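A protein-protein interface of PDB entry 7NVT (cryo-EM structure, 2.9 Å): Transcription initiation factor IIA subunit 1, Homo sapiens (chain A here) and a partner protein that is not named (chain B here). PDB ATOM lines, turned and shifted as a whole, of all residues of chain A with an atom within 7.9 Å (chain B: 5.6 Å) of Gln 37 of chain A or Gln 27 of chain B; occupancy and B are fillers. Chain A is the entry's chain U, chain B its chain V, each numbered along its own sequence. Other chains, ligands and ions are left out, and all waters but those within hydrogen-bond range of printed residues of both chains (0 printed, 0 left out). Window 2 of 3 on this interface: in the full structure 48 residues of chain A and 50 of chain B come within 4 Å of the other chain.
The backbone NH of Gln 27 of chain B is in hydrogen-bond range of the backbone carbonyl oxygen of Leu 22 of chain B (3.1 Å). OD1 of Asp 35 of chain A lies within hydrogen-bond range of N of Val 38 of chain A (3.1 Å). The backbone carbonyl oxygen (O) of Phe 29 of chain A sits at hydrogen-bond distance from the backbone NH (N) of Val 34 of chain A (3.4 Å). O of Leu 22 of chain B lies within hydrogen-bond range of OG of Ser 25 of chain B, at 2.6 Å. The side-chain carboxylate of Asp 35 of chain A sits close to the backbone NH of Gln 37 of chain A, 3.1 Å away.
Among the printed residues, merely in contact across the chains: Glu 41 of chain A with Leu 22 of chain B, Val 38 of chain A with Ile 28 of chain B, Phe 29 of chain A with Leu 32 of chain B, Leu 42 of chain A with Leu 22 of chain B, Leu 45 of chain A with Leu 22 of chain B, Val 38 of chain A with Gln 27 of chain B, Glu 41 of chain A with Gln 27 of chain B, Gln 37 of chain A with Gln 27 of chain B and Val 38 of chain A with Leu 22 of chain B.
Of the 14 printed residues of chain A, 6 touch a printed residue of chain B. Among the printed residues, 9 pairs touch across the chains. Among the printed residues, no Asp or Glu carboxylate lies within 4 Å of a Lys or Arg side-chain nitrogen of the other chain.
Of chain B, only Gln 27 (3.8 Å) comes within 4 Å of Gln 37 of chain A. Gln 27 of chain B touches three residues of chain A. Of the printed residues of chain B, Val 38 of chain A touches Leu 22, Gln 27 and Ile 28. Of the printed residues of chain B, Leu 42 of chain A touches Leu 22. Of the printed residues of chain A, Leu 22 of chain B touches Val 38, Glu 41, Leu 42 and Leu 45. Of the printed residues of chain A, Ile 28 of chain B touches Val 38 (3.5 Å). Printed residues of chain B within 4 Å of Leu 45 of chain A: Leu 22 (3.6 Å). The nearest printed residue of chain B that does not touch Gln 37 of chain A is Leu 22 of chain B (7.0 Å). The nearest printed residue of chain B that does not touch Glu 41 of chain A is Ser 25 of chain B (6.5 Å).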
ATOM      1  N   ARG A  26       0.763 -21.349  -3.714  1.00  0.00           N
ATOM      2  CA  ARG A  26       1.287 -20.212  -4.464  1.00  0.00           C
ATOM      3  C   ARG A  26       0.373 -19.860  -5.632  1.00  0.00           C
ATOM      4  O   ARG A  26       0.069 -18.685  -5.865  1.00  0.00           O
ATOM      5  CB  ARG A  26       2.700 -20.519  -4.962  1.00  0.00           C
ATOM      6  CG  ARG A  26       3.768 -20.468  -3.881  1.00  0.00           C
ATOM      7  CD  ARG A  26       4.998 -19.706  -4.348  1.00  0.00           C
ATOM      8  NE  ARG A  26       6.164 -19.983  -3.512  1.00  0.00           N
ATOM      9  CZ  ARG A  26       6.394 -19.419  -2.329  1.00  0.00           C
ATOM     10  NH1 ARG A  26       5.539 -18.537  -1.827  1.00  0.00           N
ATOM     11  NH2 ARG A  26       7.485 -19.737  -1.645  1.00  0.00           N
ATOM     12  N   PHE A  29      -2.884 -18.228  -4.344  1.00  0.00           N
ATOM     13  CA  PHE A  29      -2.687 -16.845  -3.923  1.00  0.00           C
ATOM     14  C   PHE A  29      -2.527 -15.922  -5.125  1.00  0.00           C
ATOM     15  O   PHE A  29      -3.020 -14.789  -5.115  1.00  0.00           O
ATOM     16  CB  PHE A  29      -1.472 -16.747  -2.998  1.00  0.00           C
ATOM     17  CG  PHE A  29      -1.622 -17.507  -1.704  1.00  0.00           C
ATOM     18  CD1 PHE A  29      -2.833 -18.080  -1.343  1.00  0.00           C
ATOM     19  CD2 PHE A  29      -0.546 -17.646  -0.845  1.00  0.00           C
ATOM     20  CE1 PHE A  29      -2.964 -18.775  -0.156  1.00  0.00           C
ATOM     21  CE2 PHE A  29      -0.674 -18.340   0.344  1.00  0.00           C
ATOM     22  CZ  PHE A  29      -1.883 -18.903   0.687  1.00  0.00           C
ATOM     23  N   VAL A  34      -4.508 -11.972  -4.058  1.00  0.00           N
ATOM     24  CA  VAL A  34      -3.983 -11.561  -2.760  1.00  0.00           C
ATOM     25  C   VAL A  34      -2.465 -11.517  -2.840  1.00  0.00           C
ATOM     26  O   VAL A  34      -1.839 -12.358  -3.498  1.00  0.00           O
ATOM     27  CB  VAL A  34      -4.456 -12.510  -1.642  1.00  0.00           C
ATOM     28  CG1 VAL A  34      -3.714 -12.220  -0.345  1.00  0.00           C
ATOM     29  CG2 VAL A  34      -5.958 -12.377  -1.442  1.00  0.00           C
ATOM     30  N   ASP A  35      -1.871 -10.533  -2.170  1.00  0.00           N
ATOM     31  CA  ASP A  35      -0.427 -10.354  -2.225  1.00  0.00           C
ATOM     32  C   ASP A  35       0.291 -11.560  -1.627  1.00  0.00           C
ATOM     33  O   ASP A  35      -0.188 -12.192  -0.681  1.00  0.00           O
ATOM     34  CB  ASP A  35      -0.021  -9.079  -1.485  1.00  0.00           C
ATOM     35  CG  ASP A  35      -0.400  -9.111  -0.017  1.00  0.00           C
ATOM     36  OD1 ASP A  35       0.221  -9.884   0.743  1.00  0.00           O
ATOM     37  OD2 ASP A  35      -1.318  -8.362   0.376  1.00  0.00           O
ATOM     38  N   GLU A  36       1.457 -11.874  -2.195  1.00  0.00           N
ATOM     39  CA  GLU A  36       2.239 -13.010  -1.721  1.00  0.00           C
ATOM     40  C   GLU A  36       2.757 -12.806  -0.304  1.00  0.00           C
ATOM     41  O   GLU A  36       3.118 -13.785   0.358  1.00  0.00           O
ATOM     42  CB  GLU A  36       3.410 -13.264  -2.674  1.00  0.00           C
ATOM     43  CG  GLU A  36       4.325 -14.409  -2.263  1.00  0.00           C
ATOM     44  CD  GLU A  36       3.569 -15.691  -1.975  1.00  0.00           C
ATOM     45  OE1 GLU A  36       2.571 -15.964  -2.674  1.00  0.00           O
ATOM     46  OE2 GLU A  36       3.973 -16.425  -1.050  1.00  0.00           O
ATOM     47  N   GLN A  37       2.802 -11.562   0.179  1.00  0.00           N
ATOM     48  CA  GLN A  37       3.305 -11.302   1.523  1.00  0.00           C
ATOM     49  C   GLN A  37       2.468 -11.987   2.596  1.00  0.00           C
ATOM     50  O   GLN A  37       2.958 -12.193   3.711  1.00  0.00           O
ATOM     51  CB  GLN A  37       3.348  -9.795   1.781  1.00  0.00           C
ATOM     52  CG  GLN A  37       4.026  -9.408   3.089  1.00  0.00           C
ATOM     53  CD  GLN A  37       3.045  -9.238   4.233  1.00  0.00           C
ATOM     54  OE1 GLN A  37       1.906  -8.816   4.034  1.00  0.00           O
ATOM     55  NE2 GLN A  37       3.484  -9.568   5.442  1.00  0.00           N
ATOM     56  N   VAL A  38       1.220 -12.341   2.285  1.00  0.00           N
ATOM     57  CA  VAL A  38       0.367 -13.007   3.269  1.00  0.00           C
ATOM     58  C   VAL A  38       0.963 -14.353   3.661  1.00  0.00           C
ATOM     59  O   VAL A  38       0.968 -14.731   4.838  1.00  0.00           O
ATOM     60  CB  VAL A  38      -1.062 -13.162   2.719  1.00  0.00           C
ATOM     61  CG1 VAL A  38      -1.844 -14.184   3.532  1.00  0.00           C
ATOM     62  CG2 VAL A  38      -1.777 -11.820   2.715  1.00  0.00           C
ATOM     63  N   LEU A  39       1.472 -15.098   2.678  1.00  0.00           N
ATOM     64  CA  LEU A  39       1.983 -16.438   2.950  1.00  0.00           C
ATOM     65  C   LEU A  39       3.141 -16.393   3.939  1.00  0.00           C
ATOM     66  O   LEU A  39       3.238 -17.238   4.838  1.00  0.00           O
ATOM     67  CB  LEU A  39       2.416 -17.107   1.645  1.00  0.00           C
ATOM     68  CG  LEU A  39       2.904 -18.555   1.737  1.00  0.00           C
ATOM     69  CD1 LEU A  39       2.055 -19.375   2.700  1.00  0.00           C
ATOM     70  CD2 LEU A  39       2.914 -19.196   0.357  1.00  0.00           C
ATOM     71  N   MET A  40       4.034 -15.412   3.789  1.00  0.00           N
ATOM     72  CA  MET A  40       5.169 -15.305   4.699  1.00  0.00           C
ATOM     73  C   MET A  40       4.703 -15.122   6.136  1.00  0.00           C
ATOM     74  O   MET A  40       5.248 -15.738   7.059  1.00  0.00           O
ATOM     75  CB  MET A  40       6.069 -14.142   4.276  1.00  0.00           C
ATOM     76  CG  MET A  40       6.626 -14.259   2.865  1.00  0.00           C
ATOM     77  SD  MET A  40       7.571 -15.771   2.593  1.00  0.00           S
ATOM     78  CE  MET A  40       6.337 -16.811   1.817  1.00  0.00           C
ATOM     79  N   GLU A  41       3.692 -14.278   6.346  1.00  0.00           N
ATOM     80  CA  GLU A  41       3.158 -14.079   7.689  1.00  0.00           C
ATOM     81  C   GLU A  41       2.440 -15.331   8.183  1.00  0.00           C
ATOM     82  O   GLU A  41       2.456 -15.636   9.381  1.00  0.00           O
ATOM     83  CB  GLU A  41       2.216 -12.876   7.703  1.00  0.00           C
ATOM     84  CG  GLU A  41       2.143 -12.159   9.044  1.00  0.00           C
ATOM     85  CD  GLU A  41       1.268 -12.884  10.050  1.00  0.00           C
ATOM     86  OE1 GLU A  41       0.374 -13.646   9.626  1.00  0.00           O
ATOM     87  OE2 GLU A  41       1.476 -12.689  11.266  1.00  0.00           O
ATOM     88  N   LEU A  42       1.801 -16.066   7.271  1.00  0.00           N
ATOM     89  CA  LEU A  42       1.053 -17.257   7.661  1.00  0.00           C
ATOM     90  C   LEU A  42       1.967 -18.295   8.301  1.00  0.00           C
ATOM     91  O   LEU A  42       1.635 -18.884   9.337  1.00  0.00           O
ATOM     92  CB  LEU A  42       0.343 -17.847   6.439  1.00  0.00           C
ATOM     93  CG  LEU A  42      -1.084 -17.357   6.187  1.00  0.00           C
ATOM     94  CD1 LEU A  42      -1.525 -17.704   4.773  1.00  0.00           C
ATOM     95  CD2 LEU A  42      -2.045 -17.944   7.208  1.00  0.00           C
ATOM     96  N   LYS A  43       3.131 -18.531   7.694  1.00  0.00           N
ATOM     97  CA  LYS A  43       4.052 -19.532   8.221  1.00  0.00           C
ATOM     98  C   LYS A  43       4.585 -19.122   9.588  1.00  0.00           C
ATOM     99  O   LYS A  43       4.740 -19.959  10.485  1.00  0.00           O
ATOM    100  CB  LYS A  43       5.204 -19.752   7.238  1.00  0.00           C
ATOM    101  CG  LYS A  43       6.000 -21.024   7.499  1.00  0.00           C
ATOM    102  CD  LYS A  43       7.380 -20.971   6.860  1.00  0.00           C
ATOM    103  CE  LYS A  43       7.312 -20.515   5.411  1.00  0.00           C
ATOM    104  NZ  LYS A  43       8.536 -20.890   4.651  1.00  0.00           N
ATOM    105  N   THR A  44       4.874 -17.832   9.765  1.00  0.00           N
ATOM    106  CA  THR A  44       5.426 -17.355  11.029  1.00  0.00           C
ATOM    107  C   THR A  44       4.481 -17.662  12.187  1.00  0.00           C
ATOM    108  O   THR A  44       4.881 -18.255  13.195  1.00  0.00           O
ATOM    109  CB  THR A  44       5.705 -15.852  10.944  1.00  0.00           C
ATOM    110  OG1 THR A  44       6.459 -15.567   9.758  1.00  0.00           O
ATOM    111  CG2 THR A  44       6.487 -15.383  12.164  1.00  0.00           C
ATOM    112  N   LEU A  45       3.214 -17.266  12.053  1.00  0.00           N
ATOM    113  CA  LEU A  45       2.240 -17.554  13.099  1.00  0.00           C
ATOM    114  C   LEU A  45       2.004 -19.053  13.229  1.00  0.00           C
ATOM    115  O   LEU A  45       1.816 -19.567  14.338  1.00  0.00           O
ATOM    116  CB  LEU A  45       0.927 -16.825  12.812  1.00  0.00           C
ATOM    117  CG  LEU A  45       0.943 -15.308  13.017  1.00  0.00           C
ATOM    118  CD1 LEU A  45      -0.370 -14.696  12.558  1.00  0.00           C
ATOM    119  CD2 LEU A  45       1.217 -14.955  14.471  1.00  0.00           C
ATOM    120  N   LEU B  22      -5.213 -14.220  11.322  1.00  0.00           N
ATOM    121  CA  LEU B  22      -5.133 -13.334  10.165  1.00  0.00           C
ATOM    122  C   LEU B  22      -6.497 -12.743   9.832  1.00  0.00           C
ATOM    123  O   LEU B  22      -6.601 -11.565   9.471  1.00  0.00           O
ATOM    124  CB  LEU B  22      -4.570 -14.088   8.960  1.00  0.00           C
ATOM    125  CG  LEU B  22      -3.045 -14.181   8.880  1.00  0.00           C
ATOM    126  CD1 LEU B  22      -2.522 -15.291   9.775  1.00  0.00           C
ATOM    127  CD2 LEU B  22      -2.596 -14.390   7.443  1.00  0.00           C
ATOM    128  N   ILE B  23      -7.556 -13.547   9.946  1.00  0.00           N
ATOM    129  CA  ILE B  23      -8.899 -13.052   9.659  1.00  0.00           C
ATOM    130  C   ILE B  23      -9.263 -11.922  10.612  1.00  0.00           C
ATOM    131  O   ILE B  23      -9.833 -10.903  10.202  1.00  0.00           O
ATOM    132  CB  ILE B  23      -9.920 -14.204   9.732  1.00  0.00           C
ATOM    133  CG1 ILE B  23      -9.711 -15.174   8.567  1.00  0.00           C
ATOM    134  CG2 ILE B  23     -11.340 -13.660   9.718  1.00  0.00           C
ATOM    135  CD1 ILE B  23     -10.241 -16.566   8.830  1.00  0.00           C
ATOM    136  N   SER B  25      -7.410  -9.802  11.817  1.00  0.00           N
ATOM    137  CA  SER B  25      -6.677  -8.619  11.387  1.00  0.00           C
ATOM    138  C   SER B  25      -7.119  -8.115  10.019  1.00  0.00           C
ATOM    139  O   SER B  25      -6.535  -7.152   9.513  1.00  0.00           O
ATOM    140  CB  SER B  25      -5.173  -8.914  11.361  1.00  0.00           C
ATOM    141  OG  SER B  25      -4.848  -9.810  10.314  1.00  0.00           O
ATOM    142  N   GLN B  26      -8.127  -8.739   9.412  1.00  0.00           N
ATOM    143  CA  GLN B  26      -8.635  -8.350   8.099  1.00  0.00           C
ATOM    144  C   GLN B  26      -7.593  -8.548   7.002  1.00  0.00           C
ATOM    145  O   GLN B  26      -7.666  -7.909   5.947  1.00  0.00           O
ATOM    146  CB  GLN B  26      -9.124  -6.894   8.112  1.00  0.00           C
ATOM    147  CG  GLN B  26      -9.958  -6.466   6.901  1.00  0.00           C
ATOM    148  CD  GLN B  26     -10.982  -7.504   6.482  1.00  0.00           C
ATOM    149  OE1 GLN B  26     -11.678  -8.080   7.318  1.00  0.00           O
ATOM    150  NE2 GLN B  26     -11.079  -7.748   5.180  1.00  0.00           N
ATOM    151  N   GLN B  27      -6.621  -9.429   7.230  1.00  0.00           N
ATOM    152  CA  GLN B  27      -5.573  -9.679   6.248  1.00  0.00           C
ATOM    153  C   GLN B  27      -5.985 -10.696   5.194  1.00  0.00           C
ATOM    154  O   GLN B  27      -5.505 -10.624   4.056  1.00  0.00           O
ATOM    155  CB  GLN B  27      -4.301 -10.162   6.952  1.00  0.00           C
ATOM    156  CG  GLN B  27      -3.160 -10.517   6.008  1.00  0.00           C
ATOM    157  CD  GLN B  27      -1.869 -10.817   6.742  1.00  0.00           C
ATOM    158  OE1 GLN B  27      -1.880 -11.170   7.921  1.00  0.00           O
ATOM    159  NE2 GLN B  27      -0.746 -10.676   6.047  1.00  0.00           N
ATOM    160  N   ILE B  28      -6.857 -11.639   5.539  1.00  0.00           N
ATOM    161  CA  ILE B  28      -7.294 -12.682   4.618  1.00  0.00           C
ATOM    162  C   ILE B  28      -8.804 -12.828   4.718  1.00  0.00           C
ATOM    163  O   ILE B  28      -9.370 -12.829   5.816  1.00  0.00           O
ATOM    164  CB  ILE B  28      -6.592 -14.027   4.908  1.00  0.00           C
ATOM    165  CG1 ILE B  28      -6.990 -14.559   6.289  1.00  0.00           C
ATOM    166  CG2 ILE B  28      -5.083 -13.861   4.812  1.00  0.00           C
ATOM    167  CD1 ILE B  28      -6.298 -15.852   6.671  1.00  0.00           C
ATOM    168  N   THR B  29      -9.459 -12.946   3.565  1.00  0.00           N
ATOM    169  CA  THR B  29     -10.892 -13.182   3.530  1.00  0.00           C
ATOM    170  C   THR B  29     -11.194 -14.629   3.917  1.00  0.00           C
ATOM    171  O   THR B  29     -10.344 -15.510   3.755  1.00  0.00           O
ATOM    172  CB  THR B  29     -11.443 -12.890   2.136  1.00  0.00           C
ATOM    173  OG1 THR B  29     -12.875 -12.875   2.172  1.00  0.00           O
ATOM    174  CG2 THR B  29     -10.977 -13.943   1.140  1.00  0.00           C
ATOM    175  N   LEU B  32     -10.319 -17.296   1.327  1.00  0.00           N
ATOM    176  CA  LEU B  32      -8.912 -17.665   1.199  1.00  0.00           C
ATOM    177  C   LEU B  32      -8.524 -18.713   2.233  1.00  0.00           C
ATOM    178  O   LEU B  32      -7.789 -19.658   1.924  1.00  0.00           O
ATOM    179  CB  LEU B  32      -8.033 -16.422   1.340  1.00  0.00           C
ATOM    180  CG  LEU B  32      -6.525 -16.651   1.208  1.00  0.00           C
ATOM    181  CD1 LEU B  32      -6.200 -17.350  -0.102  1.00  0.00           C
ATOM    182  CD2 LEU B  32      -5.770 -15.337   1.317  1.00  0.00           C
